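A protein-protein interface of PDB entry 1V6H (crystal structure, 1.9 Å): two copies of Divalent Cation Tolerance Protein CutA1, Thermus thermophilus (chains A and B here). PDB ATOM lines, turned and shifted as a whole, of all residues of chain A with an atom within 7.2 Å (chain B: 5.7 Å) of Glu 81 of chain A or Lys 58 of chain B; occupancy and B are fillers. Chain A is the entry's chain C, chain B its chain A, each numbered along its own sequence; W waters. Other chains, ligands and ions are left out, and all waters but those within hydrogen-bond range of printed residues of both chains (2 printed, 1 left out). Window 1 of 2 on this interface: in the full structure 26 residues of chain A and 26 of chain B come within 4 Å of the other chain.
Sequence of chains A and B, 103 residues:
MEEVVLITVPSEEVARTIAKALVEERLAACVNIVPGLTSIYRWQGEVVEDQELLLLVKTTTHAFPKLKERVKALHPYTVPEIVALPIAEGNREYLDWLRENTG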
ATOM      1  N   VAL A   5     -26.417   9.136  14.282  1.00  0.00           N
ATOM      2  CA  VAL A   5     -27.293   7.993  14.523  1.00  0.00           C
ATOM      3  C   VAL A   5     -26.508   6.695  14.657  1.00  0.00           C
ATOM      4  O   VAL A   5     -25.639   6.395  13.832  1.00  0.00           O
ATOM      5  CB  VAL A   5     -28.335   7.828  13.379  1.00  0.00           C
ATOM      6  CG1 VAL A   5     -29.076   6.501  13.523  1.00  0.00           C
ATOM      7  CG2 VAL A   5     -29.317   8.996  13.405  1.00  0.00           C
ATOM      8  N   LEU A   6     -26.831   5.930  15.698  1.00  0.00           N
ATOM      9  CA  LEU A   6     -26.177   4.653  15.954  1.00  0.00           C
ATOM     10  C   LEU A   6     -27.074   3.509  15.532  1.00  0.00           C
ATOM     11  O   LEU A   6     -28.264   3.490  15.862  1.00  0.00           O
ATOM     12  CB  LEU A   6     -25.861   4.483  17.449  1.00  0.00           C
ATOM     13  CG  LEU A   6     -25.097   5.583  18.187  1.00  0.00           C
ATOM     14  CD1 LEU A   6     -24.590   5.028  19.525  1.00  0.00           C
ATOM     15  CD2 LEU A   6     -23.958   6.069  17.360  1.00  0.00           C
ATOM     16  N   ILE A   7     -26.493   2.558  14.804  1.00  0.00           N
ATOM     17  CA  ILE A   7     -27.204   1.372  14.341  1.00  0.00           C
ATOM     18  C   ILE A   7     -26.248   0.188  14.459  1.00  0.00           C
ATOM     19  O   ILE A   7     -25.107   0.265  14.006  1.00  0.00           O
ATOM     20  CB  ILE A   7     -27.632   1.494  12.844  1.00  0.00           C
ATOM     21  CG1 ILE A   7     -28.535   2.712  12.634  1.00  0.00           C
ATOM     22  CG2 ILE A   7     -28.385   0.215  12.404  1.00  0.00           C
ATOM     23  CD1 ILE A   7     -28.763   3.032  11.151  1.00  0.00           C
ATOM     24  N   THR A   8     -26.680  -0.895  15.096  1.00  0.00           N
ATOM     25  CA  THR A   8     -25.820  -2.066  15.168  1.00  0.00           C
ATOM     26  C   THR A   8     -26.341  -3.091  14.173  1.00  0.00           C
ATOM     27  O   THR A   8     -27.549  -3.224  13.973  1.00  0.00           O
ATOM     28  CB  THR A   8     -25.759  -2.685  16.585  1.00  0.00           C
ATOM     29  OG1 THR A   8     -27.080  -2.956  17.057  1.00  0.00           O
ATOM     30  CG2 THR A   8     -25.056  -1.743  17.532  1.00  0.00           C
ATOM     31  N   VAL A   9     -25.418  -3.797  13.534  1.00  0.00           N
ATOM     32  CA  VAL A   9     -25.760  -4.796  12.533  1.00  0.00           C
ATOM     33  C   VAL A   9     -24.995  -6.080  12.805  1.00  0.00           C
ATOM     34  O   VAL A   9     -23.943  -6.063  13.443  1.00  0.00           O
ATOM     35  CB  VAL A   9     -25.435  -4.275  11.120  1.00  0.00           C
ATOM     36  CG1 VAL A   9     -26.293  -3.050  10.819  1.00  0.00           C
ATOM     37  CG2 VAL A   9     -23.966  -3.900  11.031  1.00  0.00           C
ATOM     38  N   LEU A  37     -17.653  -5.576  17.528  1.00  0.00           N
ATOM     39  CA  LEU A  37     -18.478  -5.470  18.725  1.00  0.00           C
ATOM     40  C   LEU A  37     -18.980  -6.798  19.280  1.00  0.00           C
ATOM     41  O   LEU A  37     -19.271  -7.731  18.534  1.00  0.00           O
ATOM     42  CB  LEU A  37     -19.701  -4.582  18.468  1.00  0.00           C
ATOM     43  CG  LEU A  37     -19.583  -3.070  18.642  1.00  0.00           C
ATOM     44  CD1 LEU A  37     -18.601  -2.492  17.637  1.00  0.00           C
ATOM     45  CD2 LEU A  37     -20.956  -2.455  18.452  1.00  0.00           C
ATOM     46  N   SER A  39     -22.018  -7.898  21.698  1.00  0.00           N
ATOM     47  CA  SER A  39     -23.222  -7.311  22.268  1.00  0.00           C
ATOM     48  C   SER A  39     -23.948  -8.249  23.216  1.00  0.00           C
ATOM     49  O   SER A  39     -24.148  -9.430  22.917  1.00  0.00           O
ATOM     50  CB  SER A  39     -24.166  -6.876  21.147  1.00  0.00           C
ATOM     51  OG  SER A  39     -23.566  -5.866  20.360  1.00  0.00           O
ATOM     52  N   GLU A  52     -21.448  -8.169  16.550  1.00  0.00           N
ATOM     53  CA  GLU A  52     -22.044  -7.150  15.682  1.00  0.00           C
ATOM     54  C   GLU A  52     -21.025  -6.108  15.233  1.00  0.00           C
ATOM     55  O   GLU A  52     -19.850  -6.171  15.586  1.00  0.00           O
ATOM     56  CB  GLU A  52     -23.173  -6.406  16.420  1.00  0.00           C
ATOM     57  CG  GLU A  52     -24.389  -7.235  16.826  1.00  0.00           C
ATOM     58  CD  GLU A  52     -25.483  -6.369  17.450  1.00  0.00           C
ATOM     59  OE1 GLU A  52     -25.224  -5.727  18.489  1.00  0.00           O
ATOM     60  OE2 GLU A  52     -26.602  -6.317  16.899  1.00  0.00           O
ATOM     61  N   LEU A  53     -21.510  -5.148  14.451  1.00  0.00           N
ATOM     62  CA  LEU A  53     -20.713  -4.029  13.979  1.00  0.00           C
ATOM     63  C   LEU A  53     -21.569  -2.790  14.238  1.00  0.00           C
ATOM     64  O   LEU A  53     -22.803  -2.873  14.285  1.00  0.00           O
ATOM     65  CB  LEU A  53     -20.392  -4.133  12.484  1.00  0.00           C
ATOM     66  CG  LEU A  53     -19.449  -5.258  12.046  1.00  0.00           C
ATOM     67  CD1 LEU A  53     -20.229  -6.545  11.874  1.00  0.00           C
ATOM     68  CD2 LEU A  53     -18.787  -4.882  10.737  1.00  0.00           C
ATOM     69  N   LEU A  54     -20.915  -1.649  14.397  1.00  0.00           N
ATOM     70  CA  LEU A  54     -21.613  -0.400  14.676  1.00  0.00           C
ATOM     71  C   LEU A  54     -21.523   0.619  13.553  1.00  0.00           C
ATOM     72  O   LEU A  54     -20.440   0.851  12.993  1.00  0.00           O
ATOM     73  CB  LEU A  54     -21.040   0.228  15.951  1.00  0.00           C
ATOM     74  CG  LEU A  54     -21.630   1.576  16.361  1.00  0.00           C
ATOM     75  CD1 LEU A  54     -23.076   1.382  16.802  1.00  0.00           C
ATOM     76  CD2 LEU A  54     -20.803   2.176  17.484  1.00  0.00           C
ATOM     77  N   VAL A  71     -33.695   1.800   6.764  1.00  0.00           N
ATOM     78  CA  VAL A  71     -32.901   0.886   7.589  1.00  0.00           C
ATOM     79  C   VAL A  71     -33.732  -0.366   7.889  1.00  0.00           C
ATOM     80  O   VAL A  71     -33.254  -1.495   7.751  1.00  0.00           O
ATOM     81  CB  VAL A  71     -32.473   1.548   8.920  1.00  0.00           C
ATOM     82  CG1 VAL A  71     -31.811   0.519   9.836  1.00  0.00           C
ATOM     83  CG2 VAL A  71     -31.505   2.689   8.636  1.00  0.00           C
ATOM     84  N   HIS A  75     -32.666  -4.089   7.087  1.00  0.00           N
ATOM     85  CA  HIS A  75     -32.120  -4.718   8.290  1.00  0.00           C
ATOM     86  C   HIS A  75     -32.792  -6.049   8.635  1.00  0.00           C
ATOM     87  O   HIS A  75     -34.006  -6.133   8.728  1.00  0.00           O
ATOM     88  CB  HIS A  75     -32.263  -3.745   9.477  1.00  0.00           C
ATOM     89  CG  HIS A  75     -31.250  -3.951  10.558  1.00  0.00           C
ATOM     90  ND1 HIS A  75     -31.077  -5.159  11.199  1.00  0.00           N
ATOM     91  CD2 HIS A  75     -30.341  -3.104  11.102  1.00  0.00           C
ATOM     92  CE1 HIS A  75     -30.105  -5.049  12.087  1.00  0.00           C
ATOM     93  NE2 HIS A  75     -29.642  -3.812  12.049  1.00  0.00           N
ATOM     94  N   TYR A  77     -32.900  -7.721  11.529  1.00  0.00           N
ATOM     95  CA  TYR A  77     -33.541  -7.780  12.850  1.00  0.00           C
ATOM     96  C   TYR A  77     -35.003  -7.359  12.803  1.00  0.00           C
ATOM     97  O   TYR A  77     -35.386  -6.481  12.031  1.00  0.00           O
ATOM     98  CB  TYR A  77     -32.847  -6.860  13.870  1.00  0.00           C
ATOM     99  CG  TYR A  77     -31.425  -7.215  14.259  1.00  0.00           C
ATOM    100  CD1 TYR A  77     -30.701  -6.387  15.120  1.00  0.00           C
ATOM    101  CD2 TYR A  77     -30.787  -8.344  13.741  1.00  0.00           C
ATOM    102  CE1 TYR A  77     -29.373  -6.665  15.452  1.00  0.00           C
ATOM    103  CE2 TYR A  77     -29.457  -8.635  14.068  1.00  0.00           C
ATOM    104  CZ  TYR A  77     -28.758  -7.788  14.921  1.00  0.00           C
ATOM    105  OH  TYR A  77     -27.440  -8.046  15.224  1.00  0.00           O
ATOM    106  N   VAL A  79     -36.477  -5.965  15.348  1.00  0.00           N
ATOM    107  CA  VAL A  79     -36.414  -4.662  16.003  1.00  0.00           C
ATOM    108  C   VAL A  79     -34.976  -4.149  15.948  1.00  0.00           C
ATOM    109  O   VAL A  79     -34.161  -4.472  16.809  1.00  0.00           O
ATOM    110  CB  VAL A  79     -36.853  -4.742  17.489  1.00  0.00           C
ATOM    111  CG1 VAL A  79     -36.674  -3.385  18.164  1.00  0.00           C
ATOM    112  CG2 VAL A  79     -38.309  -5.184  17.581  1.00  0.00           C
ATOM    113  N   PRO A  80     -34.640  -3.364  14.912  1.00  0.00           N
ATOM    114  CA  PRO A  80     -33.276  -2.845  14.813  1.00  0.00           C
ATOM    115  C   PRO A  80     -33.087  -1.626  15.698  1.00  0.00           C
ATOM    116  O   PRO A  80     -34.037  -0.901  15.994  1.00  0.00           O
ATOM    117  CB  PRO A  80     -33.147  -2.505  13.334  1.00  0.00           C
ATOM    118  CG  PRO A  80     -34.521  -2.020  13.009  1.00  0.00           C
ATOM    119  CD  PRO A  80     -35.414  -3.035  13.703  1.00  0.00           C
ATOM    120  N   GLU A  81     -31.851  -1.413  16.119  1.00  0.00           N
ATOM    121  CA  GLU A  81     -31.519  -0.281  16.957  1.00  0.00           C
ATOM    122  C   GLU A  81     -31.193   0.925  16.081  1.00  0.00           C
ATOM    123  O   GLU A  81     -30.244   0.897  15.307  1.00  0.00           O
ATOM    124  CB  GLU A  81     -30.318  -0.642  17.834  1.00  0.00           C
ATOM    125  CG  GLU A  81     -29.745   0.504  18.624  1.00  0.00           C
ATOM    126  CD  GLU A  81     -28.599   0.058  19.507  1.00  0.00           C
ATOM    127  OE1 GLU A  81     -27.701  -0.653  19.008  1.00  0.00           O
ATOM    128  OE2 GLU A  81     -28.594   0.415  20.699  1.00  0.00           O
ATOM    129  N   ILE A  82     -31.999   1.975  16.193  1.00  0.00           N
ATOM    130  CA  ILE A  82     -31.777   3.190  15.427  1.00  0.00           C
ATOM    131  C   ILE A  82     -31.963   4.358  16.381  1.00  0.00           C
ATOM    132  O   ILE A  82     -33.075   4.864  16.557  1.00  0.00           O
ATOM    133  CB  ILE A  82     -32.783   3.328  14.262  1.00  0.00           C
ATOM    134  CG1 ILE A  82     -32.846   2.027  13.456  1.00  0.00           C
ATOM    135  CG2 ILE A  82     -32.365   4.486  13.360  1.00  0.00           C
ATOM    136  CD1 ILE A  82     -33.919   2.041  12.344  1.00  0.00           C
ATOM    137  N   VAL A  83     -30.872   4.796  17.000  1.00  0.00           N
ATOM    138  CA  VAL A  83     -30.971   5.888  17.954  1.00  0.00           C
ATOM    139  C   VAL A  83     -30.145   7.103  17.565  1.00  0.00           C
ATOM    140  O   VAL A  83     -29.000   6.980  17.134  1.00  0.00           O
ATOM    141  CB  VAL A  83     -30.594   5.401  19.373  1.00  0.00           C
ATOM    142  CG1 VAL A  83     -31.617   4.353  19.836  1.00  0.00           C
ATOM    143  CG2 VAL A  83     -29.193   4.787  19.378  1.00  0.00           C
ATOM    144  N   GLU B   3     -31.055   6.922  27.151  1.00  0.00           N
ATOM    145  CA  GLU B   3     -29.697   7.425  26.976  1.00  0.00           C
ATOM    146  C   GLU B   3     -28.737   6.317  26.567  1.00  0.00           C
ATOM    147  O   GLU B   3     -29.015   5.132  26.759  1.00  0.00           O
ATOM    148  CB  GLU B   3     -29.182   8.032  28.289  1.00  0.00           C
ATOM    149  CG  GLU B   3     -29.998   9.190  28.849  1.00  0.00           C
ATOM    150  CD  GLU B   3     -29.542   9.618  30.246  1.00  0.00           C
ATOM    151  OE1 GLU B   3     -29.608  10.832  30.546  1.00  0.00           O
ATOM    152  OE2 GLU B   3     -29.129   8.750  31.046  1.00  0.00           O
ATOM    153  N   VAL B   4     -27.605   6.719  25.999  1.00  0.00           N
ATOM    154  CA  VAL B   4     -26.557   5.777  25.628  1.00  0.00           C
ATOM    155  C   VAL B   4     -25.446   6.163  26.593  1.00  0.00           C
ATOM    156  O   VAL B   4     -24.961   7.294  26.564  1.00  0.00           O
ATOM    157  CB  VAL B   4     -26.072   5.980  24.176  1.00  0.00           C
ATOM    158  CG1 VAL B   4     -24.803   5.147  23.926  1.00  0.00           C
ATOM    159  CG2 VAL B   4     -27.166   5.542  23.204  1.00  0.00           C
ATOM    160  N   VAL B   5     -25.071   5.249  27.476  1.00  0.00           N
ATOM    161  CA  VAL B   5     -24.031   5.562  28.450  1.00  0.00           C
ATOM    162  C   VAL B   5     -22.693   4.988  28.020  1.00  0.00           C
ATOM    163  O   VAL B   5     -22.602   3.815  27.643  1.00  0.00           O
ATOM    164  CB  VAL B   5     -24.402   5.016  29.857  1.00  0.00           C
ATOM    165  CG1 VAL B   5     -23.212   5.153  30.814  1.00  0.00           C
ATOM    166  CG2 VAL B   5     -25.600   5.782  30.400  1.00  0.00           C
ATOM    167  N   LEU B  27     -30.583  -2.962  34.361  1.00  0.00           N
ATOM    168  CA  LEU B  27     -30.132  -1.581  34.435  1.00  0.00           C
ATOM    169  C   LEU B  27     -29.835  -1.081  33.019  1.00  0.00           C
ATOM    170  O   LEU B  27     -29.563   0.102  32.796  1.00  0.00           O
ATOM    171  CB  LEU B  27     -28.884  -1.490  35.318  1.00  0.00           C
ATOM    172  CG  LEU B  27     -29.205  -1.715  36.806  1.00  0.00           C
ATOM    173  CD1 LEU B  27     -27.912  -1.774  37.610  1.00  0.00           C
ATOM    174  CD2 LEU B  27     -30.094  -0.579  37.314  1.00  0.00           C
ATOM    175  N   ALA B  28     -29.886  -2.008  32.070  1.00  0.00           N
ATOM    176  CA  ALA B  28     -29.658  -1.714  30.660  1.00  0.00           C
ATOM    177  C   ALA B  28     -30.309  -2.817  29.836  1.00  0.00           C
ATOM    178  O   ALA B  28     -30.385  -3.972  30.271  1.00  0.00           O
ATOM    179  CB  ALA B  28     -28.169  -1.657  30.370  1.00  0.00           C
ATOM    180  N   ALA B  29     -30.773  -2.468  28.640  1.00  0.00           N
ATOM    181  CA  ALA B  29     -31.414  -3.450  27.777  1.00  0.00           C
ATOM    182  C   ALA B  29     -30.373  -4.127  26.903  1.00  0.00           C
ATOM    183  O   ALA B  29     -30.538  -5.273  26.487  1.00  0.00           O
ATOM    184  CB  ALA B  29     -32.461  -2.765  26.904  1.00  0.00           C
ATOM    185  N   CYS B  30     -29.293  -3.402  26.634  1.00  0.00           N
ATOM    186  CA  CYS B  30     -28.224  -3.902  25.791  1.00  0.00           C
ATOM    187  C   CYS B  30     -26.929  -3.169  26.096  1.00  0.00           C
ATOM    188  O   CYS B  30     -26.946  -2.006  26.505  1.00  0.00           O
ATOM    189  CB  CYS B  30     -28.579  -3.686  24.313  1.00  0.00           C
ATOM    190  SG  CYS B  30     -27.170  -3.811  23.165  1.00  0.00           S
ATOM    191  N   VAL B  31     -25.812  -3.855  25.888  1.00  0.00           N
ATOM    192  CA  VAL B  31     -24.491  -3.264  26.090  1.00  0.00           C
ATOM    193  C   VAL B  31     -23.558  -3.723  24.977  1.00  0.00           C
ATOM    194  O   VAL B  31     -23.421  -4.919  24.751  1.00  0.00           O
ATOM    195  CB  VAL B  31     -23.859  -3.694  27.443  1.00  0.00           C
ATOM    196  CG1 VAL B  31     -22.411  -3.186  27.525  1.00  0.00           C
ATOM    197  CG2 VAL B  31     -24.681  -3.157  28.610  1.00  0.00           C
ATOM    198  N   ASN B  32     -22.936  -2.778  24.269  1.00  0.00           N
ATOM    199  CA  ASN B  32     -21.991  -3.129  23.209  1.00  0.00           C
ATOM    200  C   ASN B  32     -20.595  -2.912  23.756  1.00  0.00           C
ATOM    201  O   ASN B  32     -20.342  -1.925  24.450  1.00  0.00           O
ATOM    202  CB  ASN B  32     -22.128  -2.230  21.978  1.00  0.00           C
ATOM    203  CG  ASN B  32     -23.532  -2.176  21.441  1.00  0.00           C
ATOM    204  OD1 ASN B  32     -24.118  -3.197  21.069  1.00  0.00           O
ATOM    205  ND2 ASN B  32     -24.081  -0.982  21.395  1.00  0.00           N
ATOM    206  N   LEU B  56     -20.988   0.659  25.431  1.00  0.00           N
ATOM    207  CA  LEU B  56     -22.072   1.544  25.016  1.00  0.00           C
ATOM    208  C   LEU B  56     -23.302   0.908  25.665  1.00  0.00           C
ATOM    209  O   LEU B  56     -23.747  -0.161  25.259  1.00  0.00           O
ATOM    210  CB  LEU B  56     -22.217   1.560  23.485  1.00  0.00           C
ATOM    211  CG  LEU B  56     -21.011   2.050  22.657  1.00  0.00           C
ATOM    212  CD1 LEU B  56     -21.349   2.015  21.164  1.00  0.00           C
ATOM    213  CD2 LEU B  56     -20.635   3.462  23.060  1.00  0.00           C
ATOM    214  N   VAL B  57     -23.847   1.576  26.672  1.00  0.00           N
ATOM    215  CA  VAL B  57     -24.978   1.043  27.422  1.00  0.00           C
ATOM    216  C   VAL B  57     -26.306   1.699  27.044  1.00  0.00           C
ATOM    217  O   VAL B  57     -26.431   2.917  27.114  1.00  0.00           O
ATOM    218  CB  VAL B  57     -24.741   1.246  28.930  1.00  0.00           C
ATOM    219  CG1 VAL B  57     -25.812   0.506  29.734  1.00  0.00           C
ATOM    220  CG2 VAL B  57     -23.328   0.779  29.303  1.00  0.00           C
ATOM    221  N   LYS B  58     -27.289   0.899  26.642  1.00  0.00           N
ATOM    222  CA  LYS B  58     -28.603   1.444  26.280  1.00  0.00           C
ATOM    223  C   LYS B  58     -29.464   1.339  27.530  1.00  0.00           C
ATOM    224  O   LYS B  58     -29.850   0.240  27.940  1.00  0.00           O
ATOM    225  CB  LYS B  58     -29.224   0.640  25.135  1.00  0.00           C
ATOM    226  CG  LYS B  58     -28.217   0.223  24.087  1.00  0.00           C
ATOM    227  CD  LYS B  58     -27.512   1.418  23.464  1.00  0.00           C
ATOM    228  CE  LYS B  58     -26.253   0.960  22.759  1.00  0.00           C
ATOM    229  NZ  LYS B  58     -26.467  -0.281  21.957  1.00  0.00           N
ATOM    230  N   THR B  59     -29.780   2.486  28.117  1.00  0.00           N
ATOM    231  CA  THR B  59     -30.525   2.516  29.364  1.00  0.00           C
ATOM    232  C   THR B  59     -31.425   3.754  29.442  1.00  0.00           C
ATOM    233  O   THR B  59     -31.634   4.443  28.434  1.00  0.00           O
ATOM    234  CB  THR B  59     -29.510   2.496  30.554  1.00  0.00           C
ATOM    235  OG1 THR B  59     -30.202   2.479  31.806  1.00  0.00           O
ATOM    236  CG2 THR B  59     -28.604   3.709  30.499  1.00  0.00           C
ATOM    237  N   THR B  60     -31.960   4.030  30.629  1.00  0.00           N
ATOM    238  CA  THR B  60     -32.838   5.187  30.827  1.00  0.00           C
ATOM    239  C   THR B  60     -32.318   6.103  31.926  1.00  0.00           C
ATOM    240  O   THR B  60     -31.510   5.698  32.765  1.00  0.00           O
ATOM    241  CB  THR B  60     -34.279   4.756  31.187  1.00  0.00           C
ATOM    242  OG1 THR B  60     -34.281   4.082  32.455  1.00  0.00           O
ATOM    243  CG2 THR B  60     -34.828   3.822  30.131  1.00  0.00           C
ATOM    244  N   ASN B  91     -36.207   4.855  16.643  1.00  0.00           N
ATOM    245  CA  ASN B  91     -37.371   4.156  16.122  1.00  0.00           C
ATOM    246  C   ASN B  91     -38.189   3.664  17.307  1.00  0.00           C
ATOM    247  O   ASN B  91     -37.654   3.098  18.260  1.00  0.00           O
ATOM    248  CB  ASN B  91     -36.986   3.006  15.179  1.00  0.00           C
ATOM    249  CG  ASN B  91     -36.071   1.983  15.816  1.00  0.00           C
ATOM    250  OD1 ASN B  91     -36.280   0.781  15.653  1.00  0.00           O
ATOM    251  ND2 ASN B  91     -35.039   2.443  16.510  1.00  0.00           N
ATOM    252  N   TYR B  94     -37.915   0.127  18.911  1.00  0.00           N
ATOM    253  CA  TYR B  94     -36.691  -0.051  19.677  1.00  0.00           C
ATOM    254  C   TYR B  94     -36.784   0.613  21.046  1.00  0.00           C
ATOM    255  O   TYR B  94     -36.431   0.007  22.061  1.00  0.00           O
ATOM    256  CB  TYR B  94     -35.486   0.527  18.927  1.00  0.00           C
ATOM    257  CG  TYR B  94     -34.232   0.467  19.763  1.00  0.00           C
ATOM    258  CD1 TYR B  94     -33.525  -0.729  19.903  1.00  0.00           C
ATOM    259  CD2 TYR B  94     -33.804   1.578  20.492  1.00  0.00           C
ATOM    260  CE1 TYR B  94     -32.429  -0.822  20.756  1.00  0.00           C
ATOM    261  CE2 TYR B  94     -32.707   1.495  21.352  1.00  0.00           C
ATOM    262  CZ  TYR B  94     -32.030   0.288  21.479  1.00  0.00           C
ATOM    263  OH  TYR B  94     -30.971   0.178  22.351  1.00  0.00           O
ATOM    264  N   TRP B  97     -38.935  -1.293  23.325  1.00  0.00           N
ATOM    265  CA  TRP B  97     -38.199  -2.470  23.762  1.00  0.00           C
ATOM    266  C   TRP B  97     -37.218  -2.105  24.881  1.00  0.00           C
ATOM    267  O   TRP B  97     -37.125  -2.801  25.902  1.00  0.00           O
ATOM    268  CB  TRP B  97     -37.438  -3.063  22.575  1.00  0.00           C
ATOM    269  CG  TRP B  97     -36.490  -4.168  22.924  1.00  0.00           C
ATOM    270  CD1 TRP B  97     -36.786  -5.494  23.073  1.00  0.00           C
ATOM    271  CD2 TRP B  97     -35.083  -4.041  23.157  1.00  0.00           C
ATOM    272  NE1 TRP B  97     -35.650  -6.201  23.379  1.00  0.00           N
ATOM    273  CE2 TRP B  97     -34.588  -5.334  23.440  1.00  0.00           C
ATOM    274  CE3 TRP B  97     -34.189  -2.959  23.155  1.00  0.00           C
ATOM    275  CZ2 TRP B  97     -33.238  -5.578  23.719  1.00  0.00           C
ATOM    276  CZ3 TRP B  97     -32.841  -3.202  23.430  1.00  0.00           C
ATOM    277  CH2 TRP B  97     -32.382  -4.502  23.709  1.00  0.00           C
ATOM    278  N   LEU B  98     -36.489  -1.013  24.683  1.00  0.00           N
ATOM    279  CA  LEU B  98     -35.519  -0.561  25.671  1.00  0.00           C
ATOM    280  C   LEU B  98     -36.225  -0.317  27.000  1.00  0.00           C
ATOM    281  O   LEU B  98     -35.777  -0.787  28.045  1.00  0.00           O
ATOM    282  CB  LEU B  98     -34.827   0.719  25.189  1.00  0.00           C
ATOM    283  CG  LEU B  98     -33.616   1.228  25.984  1.00  0.00           C
ATOM    284  CD1 LEU B  98     -32.883   2.275  25.169  1.00  0.00           C
ATOM    285  CD2 LEU B  98     -34.063   1.814  27.304  1.00  0.00           C
ATOM    286  N   THR B 102     -35.858  -2.598  30.789  1.00  0.00           N
ATOM    287  CA  THR B 102     -35.085  -1.879  31.794  1.00  0.00           C
ATOM    288  C   THR B 102     -36.044  -1.642  32.964  1.00  0.00           C
ATOM    289  O   THR B 102     -37.258  -1.557  32.762  1.00  0.00           O
ATOM    290  CB  THR B 102     -34.520  -0.530  31.258  1.00  0.00           C
ATOM    291  OG1 THR B 102     -35.576   0.273  30.714  1.00  0.00           O
ATOM    292  CG2 THR B 102     -33.476  -0.789  30.177  1.00  0.00           C
HETATM  293  O   HOH W   1     -25.360   1.361  19.827  1.00  0.00           O
HETATM  294  O   HOH W   2     -29.985  -2.428  21.677  1.00  0.00           O
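The side-chain amide oxygen (OD1) of Asn 32 of chain B is in hydrogen-bond range of the side-chain hydroxyl (OG) of Ser 39 of chain A (2.8 Å). NZ of Lys 58 of chain B lies within salt-bridge range of OE2 of Glu 81 of chain A, 2.6 Å away. OD1 of Asn 91 of chain B lies close to O of Pro 80 of chain A. N of Ile 82 of chain A lies close to ND2 of Asn 91 of chain B (3.1 Å). The side-chain hydroxyl (OH) of Tyr 94 of chain B is in hydrogen-bond range of the side-chain carboxylate (OE2) of Glu 81 of chain A (2.9 Å).
N of Ala 29 of chain B sits at hydrogen-bond distance from O of Lys 58 of chain B, 2.9 Å away. The side-chain sulfur of Cys 30 of chain B lies within hydrogen-bond range of the side-chain amide oxygen of Asn 32 of chain B (3.8 Å). N of Lys 58 of chain B sits at hydrogen-bond distance from O of Cys 30 of chain B (2.9 Å). N of Leu 56 of chain B is in hydrogen-bond range of O of Asn 32 of chain B, 2.8 Å away. NZ of Lys 58 of chain B sits close to ND2 of Asn 32 of chain B, 2.5 Å away. OG1 of Thr 8 of chain A sits at hydrogen-bond distance from OE2 of Glu 52 of chain A (3.4 Å).
Among the printed residues, merely in contact across the chains: Thr 8 of chain A with Asn 32 of chain B (3.9 Å), Leu 37 of chain A with Asn 32 of chain B (3.7 Å), Ser 39 of chain A with Val 31 of chain B (3.5 Å), Glu 52 of chain A with Asn 32 of chain B (3.8 Å), Leu 54 of chain A with Leu 56 of chain B (3.7 Å), Val 79 of chain A with Tyr 94 of chain B (3.7 Å), Pro 80 of chain A with Tyr 94 of chain B (3.6 Å) and Val 83 of chain A with Tyr 94 of chain B (3.4 Å).
Printed residues of chain B within 4 Å of Thr 8 of chain A: Asn 32 (3.9 Å). Glu 81 of chain A touches just these residues of chain B: Lys 58 (2.6 Å) and Tyr 94 (2.9 Å). Printed residues of chain B within 4 Å of Ile 82 of chain A: Asn 91 (3.1 Å). Of the printed residues of chain B, Val 83 of chain A touches Tyr 94 (3.4 Å). Ala 28 of chain B touches none of the printed residues of chain A. Cys 30 of chain B touches none of the printed residues of chain A. Of the printed residues of chain A, Leu 56 of chain B touches Leu 54 (3.7 Å). Of chain A, only Glu 81 (2.6 Å) comes within 4 Å of Lys 58 of chain B. Printed residues of chain A within 4 Å of Tyr 94 of chain B: Val 79, Pro 80, Glu 81 and Val 83. The nearest residue of chain A that does not touch Lys 58 of chain B is Thr 8 of chain A (4.9 Å). The nearest printed residue of chain B that does not touch Leu 54 of chain A is Asn 32 of chain B (5.3 Å).
Hydrophobic or aromatic side chains of chain A within 4 Å of the printed part of chain B: Leu 37, Leu 54, Val 79, Ile 82 and Val 83. Printed residues of chain B that touch a printed residue of chain A: Val 31, Asn 32, Leu 56, Lys 58, Asn 91 and Tyr 94. Among the printed residues, 13 pairs touch across the chains.
Position printed for both chains: 5. Of the 13 pairs that touch across the chains among the printed residues, none has its exchanged pair printed and touching as well.
Water W2 lies within hydrogen-bond range of OH of Tyr 94 of chain B (2.9 Å), OE2 of Glu 81 of chain A (3.3 Å) and SG of Cys 30 of chain B (3.5 Å). Water W1 lies within hydrogen-bond range of NZ of Lys 58 of chain B (2.9 Å), ND2 of Asn 32 of chain B (3.1 Å) and OE1 of Glu 81 of chain A (3.2 Å).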
